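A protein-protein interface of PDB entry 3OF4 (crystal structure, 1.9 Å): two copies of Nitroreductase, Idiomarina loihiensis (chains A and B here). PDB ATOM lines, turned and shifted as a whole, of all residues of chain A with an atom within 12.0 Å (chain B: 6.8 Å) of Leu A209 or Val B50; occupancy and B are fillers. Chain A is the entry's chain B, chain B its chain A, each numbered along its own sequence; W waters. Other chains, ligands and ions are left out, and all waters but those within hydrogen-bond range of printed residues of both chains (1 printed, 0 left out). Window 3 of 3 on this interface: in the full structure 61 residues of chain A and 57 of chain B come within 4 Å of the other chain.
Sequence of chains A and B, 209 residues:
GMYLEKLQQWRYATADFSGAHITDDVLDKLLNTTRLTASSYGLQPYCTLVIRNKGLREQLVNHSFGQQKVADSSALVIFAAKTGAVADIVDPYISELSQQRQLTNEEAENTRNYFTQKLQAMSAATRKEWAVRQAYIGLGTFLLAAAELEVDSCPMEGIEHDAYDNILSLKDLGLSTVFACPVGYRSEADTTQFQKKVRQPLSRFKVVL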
ATOM      1  N   PRO A 201     -22.068  23.488  26.258  1.00  0.00           N
ATOM      2  CA  PRO A 201     -21.956  24.815  26.878  1.00  0.00           C
ATOM      3  C   PRO A 201     -20.732  25.561  26.365  1.00  0.00           C
ATOM      4  O   PRO A 201     -19.789  24.943  25.848  1.00  0.00           O
ATOM      5  CB  PRO A 201     -21.792  24.524  28.346  1.00  0.00           C
ATOM      6  CG  PRO A 201     -21.530  23.004  28.449  1.00  0.00           C
ATOM      7  CD  PRO A 201     -21.838  22.365  27.188  1.00  0.00           C
ATOM      8  N   LEU A 202     -20.724  26.875  26.542  1.00  0.00           N
ATOM      9  CA  LEU A 202     -19.598  27.664  26.068  1.00  0.00           C
ATOM     10  C   LEU A 202     -18.279  27.232  26.727  1.00  0.00           C
ATOM     11  O   LEU A 202     -17.244  27.272  26.081  1.00  0.00           O
ATOM     12  CB  LEU A 202     -19.873  29.171  26.277  1.00  0.00           C
ATOM     13  CG  LEU A 202     -18.941  30.164  25.572  1.00  0.00           C
ATOM     14  CD1 LEU A 202     -19.095  30.060  24.080  1.00  0.00           C
ATOM     15  CD2 LEU A 202     -19.253  31.593  26.096  1.00  0.00           C
ATOM     16  N   SER A 203     -18.302  26.770  27.977  1.00  0.00           N
ATOM     17  CA  SER A 203     -17.059  26.377  28.661  1.00  0.00           C
ATOM     18  C   SER A 203     -16.399  25.174  27.981  1.00  0.00           C
ATOM     19  O   SER A 203     -15.207  24.967  28.140  1.00  0.00           O
ATOM     20  CB  SER A 203     -17.319  26.048  30.123  1.00  0.00           C
ATOM     21  OG  SER A 203     -18.306  25.029  30.209  1.00  0.00           O
ATOM     22  N   ARG A 204     -17.171  24.401  27.216  1.00  0.00           N
ATOM     23  CA  ARG A 204     -16.604  23.267  26.485  1.00  0.00           C
ATOM     24  C   ARG A 204     -16.363  23.649  25.024  1.00  0.00           C
ATOM     25  O   ARG A 204     -15.350  23.272  24.465  1.00  0.00           O
ATOM     26  CB  ARG A 204     -17.503  22.014  26.584  1.00  0.00           C
ATOM     27  CG  ARG A 204     -17.607  21.375  27.965  1.00  0.00           C
ATOM     28  CD  ARG A 204     -18.136  19.899  27.855  1.00  0.00           C
ATOM     29  N   PHE A 205     -17.252  24.460  24.443  1.00  0.00           N
ATOM     30  CA  PHE A 205     -17.212  24.797  23.032  1.00  0.00           C
ATOM     31  C   PHE A 205     -16.082  25.769  22.710  1.00  0.00           C
ATOM     32  O   PHE A 205     -15.513  25.700  21.617  1.00  0.00           O
ATOM     33  CB  PHE A 205     -18.536  25.426  22.611  1.00  0.00           C
ATOM     34  CG  PHE A 205     -18.645  25.698  21.130  1.00  0.00           C
ATOM     35  CD1 PHE A 205     -18.914  24.675  20.257  1.00  0.00           C
ATOM     36  CD2 PHE A 205     -18.483  26.984  20.616  1.00  0.00           C
ATOM     37  CE1 PHE A 205     -19.029  24.916  18.871  1.00  0.00           C
ATOM     38  CE2 PHE A 205     -18.601  27.246  19.238  1.00  0.00           C
ATOM     39  CZ  PHE A 205     -18.883  26.200  18.376  1.00  0.00           C
ATOM     40  N   LYS A 206     -15.794  26.693  23.622  1.00  0.00           N
ATOM     41  CA  LYS A 206     -14.692  27.636  23.460  1.00  0.00           C
ATOM     42  C   LYS A 206     -13.501  27.072  24.193  1.00  0.00           C
ATOM     43  O   LYS A 206     -13.615  26.761  25.364  1.00  0.00           O
ATOM     44  CB  LYS A 206     -15.059  29.023  24.009  1.00  0.00           C
ATOM     45  CG  LYS A 206     -13.881  29.993  24.192  1.00  0.00           C
ATOM     46  CD  LYS A 206     -14.334  31.285  24.828  1.00  0.00           C
ATOM     47  CE  LYS A 206     -13.264  32.353  24.660  1.00  0.00           C
ATOM     48  NZ  LYS A 206     -13.153  33.313  25.780  1.00  0.00           N
ATOM     49  N   VAL A 207     -12.368  26.961  23.504  1.00  0.00           N
ATOM     50  CA  VAL A 207     -11.127  26.466  24.108  1.00  0.00           C
ATOM     51  C   VAL A 207     -10.106  27.554  23.908  1.00  0.00           C
ATOM     52  O   VAL A 207      -9.752  27.887  22.775  1.00  0.00           O
ATOM     53  CB  VAL A 207     -10.624  25.224  23.399  1.00  0.00           C
ATOM     54  CG1 VAL A 207      -9.305  24.793  23.994  1.00  0.00           C
ATOM     55  CG2 VAL A 207     -11.722  24.139  23.418  1.00  0.00           C
ATOM     56  N   VAL A 208      -9.684  28.159  24.997  1.00  0.00           N
ATOM     57  CA  VAL A 208      -8.679  29.191  24.945  1.00  0.00           C
ATOM     58  C   VAL A 208      -7.285  28.547  24.918  1.00  0.00           C
ATOM     59  O   VAL A 208      -6.901  27.785  25.814  1.00  0.00           O
ATOM     60  CB  VAL A 208      -8.818  30.173  26.138  1.00  0.00           C
ATOM     61  CG1 VAL A 208      -7.758  31.295  26.051  1.00  0.00           C
ATOM     62  CG2 VAL A 208     -10.249  30.730  26.245  1.00  0.00           C
ATOM     63  N   LEU A 209      -6.509  28.859  23.888  1.00  0.00           N
ATOM     64  CA  LEU A 209      -5.149  28.391  23.838  1.00  0.00           C
ATOM     65  C   LEU A 209      -4.298  29.593  24.158  1.00  0.00           C
ATOM     66  O   LEU A 209      -4.753  30.723  23.969  1.00  0.00           O
ATOM     67  CB  LEU A 209      -4.813  27.794  22.465  1.00  0.00           C
ATOM     68  CG  LEU A 209      -5.432  26.421  22.211  1.00  0.00           C
ATOM     69  CD1 LEU A 209      -5.229  26.050  20.771  1.00  0.00           C
ATOM     70  CD2 LEU A 209      -4.812  25.421  23.141  1.00  0.00           C
ATOM     71  OXT LEU A 209      -3.189  29.472  24.635  1.00  0.00           O
ATOM     72  N   ASP B  24     -13.256  40.206  25.171  1.00  0.00           N
ATOM     73  CA  ASP B  24     -13.755  38.873  25.482  1.00  0.00           C
ATOM     74  C   ASP B  24     -15.258  38.812  25.501  1.00  0.00           C
ATOM     75  O   ASP B  24     -15.785  37.806  25.069  1.00  0.00           O
ATOM     76  CB  ASP B  24     -13.221  38.380  26.818  1.00  0.00           C
ATOM     77  CG  ASP B  24     -11.764  37.951  26.743  1.00  0.00           C
ATOM     78  OD1 ASP B  24     -11.265  37.650  25.638  1.00  0.00           O
ATOM     79  OD2 ASP B  24     -11.129  37.897  27.813  1.00  0.00           O
ATOM     80  N   LEU B  27     -16.277  38.627  21.841  1.00  0.00           N
ATOM     81  CA  LEU B  27     -15.917  37.310  21.299  1.00  0.00           C
ATOM     82  C   LEU B  27     -16.810  36.201  21.876  1.00  0.00           C
ATOM     83  O   LEU B  27     -17.237  35.300  21.143  1.00  0.00           O
ATOM     84  CB  LEU B  27     -14.433  36.988  21.481  1.00  0.00           C
ATOM     85  CG  LEU B  27     -13.890  35.802  20.655  1.00  0.00           C
ATOM     86  CD1 LEU B  27     -14.065  36.024  19.144  1.00  0.00           C
ATOM     87  CD2 LEU B  27     -12.418  35.547  20.978  1.00  0.00           C
ATOM     88  N   ASP B  28     -17.162  36.300  23.157  1.00  0.00           N
ATOM     89  CA  ASP B  28     -18.085  35.327  23.767  1.00  0.00           C
ATOM     90  C   ASP B  28     -19.514  35.383  23.204  1.00  0.00           C
ATOM     91  O   ASP B  28     -20.183  34.341  23.097  1.00  0.00           O
ATOM     92  CB  ASP B  28     -18.173  35.540  25.286  1.00  0.00           C
ATOM     93  CG  ASP B  28     -16.984  34.951  26.049  1.00  0.00           C
ATOM     94  OD1 ASP B  28     -16.089  34.326  25.448  1.00  0.00           O
ATOM     95  OD2 ASP B  28     -16.970  35.132  27.277  1.00  0.00           O
ATOM     96  N   LEU B  31     -19.141  33.539  19.849  1.00  0.00           N
ATOM     97  CA  LEU B  31     -19.018  32.078  20.022  1.00  0.00           C
ATOM     98  C   LEU B  31     -20.259  31.432  20.642  1.00  0.00           C
ATOM     99  O   LEU B  31     -20.580  30.291  20.328  1.00  0.00           O
ATOM    100  CB  LEU B  31     -17.739  31.739  20.810  1.00  0.00           C
ATOM    101  CG  LEU B  31     -16.422  32.194  20.137  1.00  0.00           C
ATOM    102  CD1 LEU B  31     -15.203  31.880  21.034  1.00  0.00           C
ATOM    103  CD2 LEU B  31     -16.255  31.565  18.773  1.00  0.00           C
ATOM    104  N   THR B  48     -14.303  25.615  18.852  1.00  0.00           N
ATOM    105  CA  THR B  48     -13.560  26.784  18.388  1.00  0.00           C
ATOM    106  C   THR B  48     -12.414  27.099  19.337  1.00  0.00           C
ATOM    107  O   THR B  48     -12.645  27.321  20.542  1.00  0.00           O
ATOM    108  CB  THR B  48     -14.494  28.012  18.322  1.00  0.00           C
ATOM    109  OG1 THR B  48     -15.106  28.228  19.581  1.00  0.00           O
ATOM    110  CG2 THR B  48     -15.600  27.818  17.322  1.00  0.00           C
ATOM    111  N   LEU B  49     -11.187  27.146  18.822  1.00  0.00           N
ATOM    112  CA  LEU B  49     -10.027  27.514  19.610  1.00  0.00           C
ATOM    113  C   LEU B  49      -9.837  29.004  19.450  1.00  0.00           C
ATOM    114  O   LEU B  49     -10.017  29.509  18.339  1.00  0.00           O
ATOM    115  CB  LEU B  49      -8.808  26.759  19.111  1.00  0.00           C
ATOM    116  CG  LEU B  49      -8.991  25.249  18.921  1.00  0.00           C
ATOM    117  CD1 LEU B  49      -7.759  24.669  18.246  1.00  0.00           C
ATOM    118  CD2 LEU B  49      -9.282  24.543  20.257  1.00  0.00           C
ATOM    119  N   VAL B  50      -9.535  29.714  20.537  1.00  0.00           N
ATOM    120  CA  VAL B  50      -9.288  31.177  20.492  1.00  0.00           C
ATOM    121  C   VAL B  50      -7.819  31.471  20.856  1.00  0.00           C
ATOM    122  O   VAL B  50      -7.353  31.102  21.952  1.00  0.00           O
ATOM    123  CB  VAL B  50     -10.217  31.919  21.460  1.00  0.00           C
ATOM    124  CG1 VAL B  50      -9.900  33.460  21.535  1.00  0.00           C
ATOM    125  CG2 VAL B  50     -11.632  31.703  21.120  1.00  0.00           C
ATOM    126  N   ILE B  51      -7.091  32.133  19.956  1.00  0.00           N
ATOM    127  CA  ILE B  51      -5.709  32.496  20.180  1.00  0.00           C
ATOM    128  C   ILE B  51      -5.469  33.991  19.958  1.00  0.00           C
ATOM    129  O   ILE B  51      -5.805  34.530  18.903  1.00  0.00           O
ATOM    130  CB  ILE B  51      -4.759  31.786  19.198  1.00  0.00           C
ATOM    131  CG1 ILE B  51      -4.917  30.271  19.254  1.00  0.00           C
ATOM    132  CG2 ILE B  51      -3.326  32.174  19.500  1.00  0.00           C
ATOM    133  CD1 ILE B  51      -4.055  29.605  18.209  1.00  0.00           C
ATOM    134  N   ARG B  52      -4.835  34.635  20.928  1.00  0.00           N
ATOM    135  CA  ARG B  52      -4.458  36.055  20.798  1.00  0.00           C
ATOM    136  C   ARG B  52      -2.945  36.287  20.658  1.00  0.00           C
ATOM    137  O   ARG B  52      -2.527  37.233  19.998  1.00  0.00           O
ATOM    138  CB  ARG B  52      -5.005  36.855  21.973  1.00  0.00           C
ATOM    139  CG  ARG B  52      -6.518  37.028  21.976  1.00  0.00           C
ATOM    140  CD  ARG B  52      -6.945  37.652  23.290  1.00  0.00           C
ATOM    141  NE  ARG B  52      -8.378  37.874  23.420  1.00  0.00           N
ATOM    142  CZ  ARG B  52      -9.068  38.886  22.879  1.00  0.00           C
ATOM    143  NH1 ARG B  52      -8.470  39.802  22.116  1.00  0.00           N
ATOM    144  NH2 ARG B  52     -10.377  38.978  23.096  1.00  0.00           N
ATOM    145  N   ASN B  53      -2.145  35.407  21.262  1.00  0.00           N
ATOM    146  CA  ASN B  53      -0.679  35.475  21.229  1.00  0.00           C
ATOM    147  C   ASN B  53      -0.150  35.877  19.869  1.00  0.00           C
ATOM    148  O   ASN B  53      -0.467  35.238  18.860  1.00  0.00           O
ATOM    149  CB  ASN B  53      -0.110  34.118  21.568  1.00  0.00           C
ATOM    150  CG  ASN B  53       1.350  34.168  21.906  1.00  0.00           C
ATOM    151  OD1 ASN B  53       2.208  34.600  21.100  1.00  0.00           O
ATOM    152  ND2 ASN B  53       1.652  33.754  23.123  1.00  0.00           N
ATOM    153  N   LEU B  56       3.170  33.273  18.294  1.00  0.00           N
ATOM    154  CA  LEU B  56       2.492  32.070  17.831  1.00  0.00           C
ATOM    155  C   LEU B  56       1.765  32.218  16.497  1.00  0.00           C
ATOM    156  O   LEU B  56       1.793  31.304  15.650  1.00  0.00           O
ATOM    157  CB  LEU B  56       1.446  31.622  18.857  1.00  0.00           C
ATOM    158  CG  LEU B  56       0.870  30.230  18.587  1.00  0.00           C
ATOM    159  CD1 LEU B  56       1.944  29.217  18.121  1.00  0.00           C
ATOM    160  CD2 LEU B  56       0.114  29.715  19.842  1.00  0.00           C
ATOM    161  N   ALA B  75      -7.824  38.742  17.429  1.00  0.00           N
ATOM    162  CA  ALA B  75      -7.890  37.343  17.898  1.00  0.00           C
ATOM    163  C   ALA B  75      -8.007  36.433  16.703  1.00  0.00           C
ATOM    164  O   ALA B  75      -8.445  36.861  15.629  1.00  0.00           O
ATOM    165  CB  ALA B  75      -9.088  37.128  18.830  1.00  0.00           C
ATOM    166  N   LEU B  76      -7.630  35.172  16.892  1.00  0.00           N
ATOM    167  CA  LEU B  76      -7.787  34.150  15.852  1.00  0.00           C
ATOM    168  C   LEU B  76      -8.706  33.057  16.396  1.00  0.00           C
ATOM    169  O   LEU B  76      -8.495  32.542  17.514  1.00  0.00           O
ATOM    170  CB  LEU B  76      -6.433  33.555  15.421  1.00  0.00           C
ATOM    171  CG  LEU B  76      -6.373  32.546  14.246  1.00  0.00           C
ATOM    172  CD1 LEU B  76      -6.807  33.133  12.896  1.00  0.00           C
ATOM    173  CD2 LEU B  76      -4.909  31.897  14.175  1.00  0.00           C
ATOM    174  N   VAL B  77      -9.757  32.753  15.643  1.00  0.00           N
ATOM    175  CA  VAL B  77     -10.655  31.656  16.028  1.00  0.00           C
ATOM    176  C   VAL B  77     -10.354  30.510  15.082  1.00  0.00           C
ATOM    177  O   VAL B  77     -10.445  30.679  13.863  1.00  0.00           O
ATOM    178  CB  VAL B  77     -12.134  32.055  15.973  1.00  0.00           C
ATOM    179  CG1 VAL B  77     -13.083  30.835  16.231  1.00  0.00           C
ATOM    180  CG2 VAL B  77     -12.444  33.172  17.004  1.00  0.00           C
ATOM    181  N   ILE B  78     -10.049  29.328  15.607  1.00  0.00           N
ATOM    182  CA  ILE B  78      -9.798  28.162  14.743  1.00  0.00           C
ATOM    183  C   ILE B  78     -10.932  27.182  14.985  1.00  0.00           C
ATOM    184  O   ILE B  78     -11.161  26.807  16.122  1.00  0.00           O
ATOM    185  CB  ILE B  78      -8.422  27.482  15.030  1.00  0.00           C
ATOM    186  CG1 ILE B  78      -7.277  28.447  14.675  1.00  0.00           C
ATOM    187  CG2 ILE B  78      -8.278  26.155  14.220  1.00  0.00           C
ATOM    188  CD1 ILE B  78      -5.988  28.132  15.321  1.00  0.00           C
ATOM    189  N   LEU B 168       0.166  23.799  17.151  1.00  0.00           N
ATOM    190  CA  LEU B 168      -0.777  23.951  18.275  1.00  0.00           C
ATOM    191  C   LEU B 168      -1.008  22.682  19.136  1.00  0.00           C
ATOM    192  O   LEU B 168      -1.831  22.707  20.052  1.00  0.00           O
ATOM    193  CB  LEU B 168      -2.131  24.432  17.747  1.00  0.00           C
ATOM    194  CG  LEU B 168      -2.108  25.716  16.933  1.00  0.00           C
ATOM    195  CD1 LEU B 168      -3.467  26.018  16.391  1.00  0.00           C
ATOM    196  CD2 LEU B 168      -1.607  26.895  17.801  1.00  0.00           C
ATOM    197  N   LEU B 170      -2.439  19.732  18.524  1.00  0.00           N
ATOM    198  CA  LEU B 170      -3.845  19.390  18.530  1.00  0.00           C
ATOM    199  C   LEU B 170      -4.095  17.888  18.606  1.00  0.00           C
ATOM    200  O   LEU B 170      -5.146  17.481  19.126  1.00  0.00           O
ATOM    201  CB  LEU B 170      -4.583  20.007  17.335  1.00  0.00           C
ATOM    202  CG  LEU B 170      -4.648  21.533  17.315  1.00  0.00           C
ATOM    203  CD1 LEU B 170      -5.651  22.023  16.216  1.00  0.00           C
ATOM    204  CD2 LEU B 170      -5.043  22.074  18.697  1.00  0.00           C
ATOM    205  N   LEU B 173      -5.018  16.728  21.945  1.00  0.00           N
ATOM    206  CA  LEU B 173      -6.416  17.054  22.341  1.00  0.00           C
ATOM    207  C   LEU B 173      -7.481  16.329  21.497  1.00  0.00           C
ATOM    208  O   LEU B 173      -8.676  16.524  21.718  1.00  0.00           O
ATOM    209  CB  LEU B 173      -6.646  18.567  22.259  1.00  0.00           C
ATOM    210  CG  LEU B 173      -5.573  19.477  22.855  1.00  0.00           C
ATOM    211  CD1 LEU B 173      -5.819  20.958  22.548  1.00  0.00           C
ATOM    212  CD2 LEU B 173      -5.407  19.203  24.368  1.00  0.00           C
ATOM    213  N   VAL B 183     -10.460  37.556  13.697  1.00  0.00           N
ATOM    214  CA  VAL B 183     -11.546  38.437  14.056  1.00  0.00           C
ATOM    215  C   VAL B 183     -10.991  39.739  14.643  1.00  0.00           C
ATOM    216  O   VAL B 183      -9.894  39.777  15.222  1.00  0.00           O
ATOM    217  CB  VAL B 183     -12.527  37.794  15.085  1.00  0.00           C
ATOM    218  CG1 VAL B 183     -13.335  36.641  14.458  1.00  0.00           C
ATOM    219  CG2 VAL B 183     -11.753  37.333  16.314  1.00  0.00           C
HETATM  220  O   HOH W   1      -6.756  33.441  23.434  1.00  0.00           O
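Printed residues of chain A that touch a printed residue of chain B: Leu A202, Phe A205, Lys A206, Val A207, Val A208 and Leu A209. Of the 19 printed residues of chain B, 5 touch a printed residue of chain A. Hydrophobic or aromatic side chains of chain B within 4 Å of the printed part of chain A: Leu B31, Leu B49 and Val B50. Among the printed residues, 13 pairs touch across the chains.
Leu A209 touches two residues of chain B. No residue of chain A comes within 4 Å of Ile B51. No residue of chain A comes within 4 Å of Ala B75. No residue of chain A comes within 4 Å of Leu B168. Printed residues of chain B within 4 Å of Val A207: Thr B48, Leu B49 and Val B50. Of the printed residues of chain A, Asp B28 touches Lys A206 (3.1 Å). Printed residues of chain B within 4 Å of Lys A206: Asp B28, Leu B31, Thr B48 and Val B50. Printed residues of chain B within 4 Å of Leu A202: Leu B31. Ser A203 touches none of the printed residues of chain B. Asp B24 touches none of the printed residues of chain A. The nearest residue of chain B that does not touch Leu A209 is Ile B51 (4.1 Å). The nearest residue of chain A that does not touch Val B50 is Phe A205 (7.2 Å). The nearest printed residue of chain B that does not touch Val A207 is Leu B173 (5.4 Å).
The backbone NH of Val B50 lies within hydrogen-bond range of the backbone carbonyl oxygen of Val A207 (2.9 Å). The backbone carbonyl oxygen of Thr B48 sits at hydrogen-bond distance from the backbone NH of Val A207 (3.0 Å). N of Thr B48 is in hydrogen-bond range of O of Phe A205. The backbone carbonyl oxygen (O) of Val B50 is in hydrogen-bond range of the backbone NH (N) of Leu A209 (3.1 Å). OD1 of Asp B28 lies within salt-bridge range of NZ of Lys A206, 3.1 Å away.
No position is printed for both chains.
Water W1 lies within hydrogen-bond range of O of Val B50 (2.8 Å), N of Arg B52 (3.4 Å) and O of Leu A209 (3.4 Å).
N of Leu B49 sits at hydrogen-bond distance from O of Ile B78 (2.7 Å).
Leu B31 touches Leu A202 (C to CD1, 3.9 Å). Leu B31 touches Phe A205 (O to CE2, 3.8 Å). Lys A206 touches Leu B31. Lys A206 touches Thr B48 (CA to O, 3.6 Å). CE of Lys A206 touches CG2 of Val B50, 3.95 Å away. Val A207 touches Leu B49. Val A208 touches Val B50. Leu A209 touches Leu B49.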
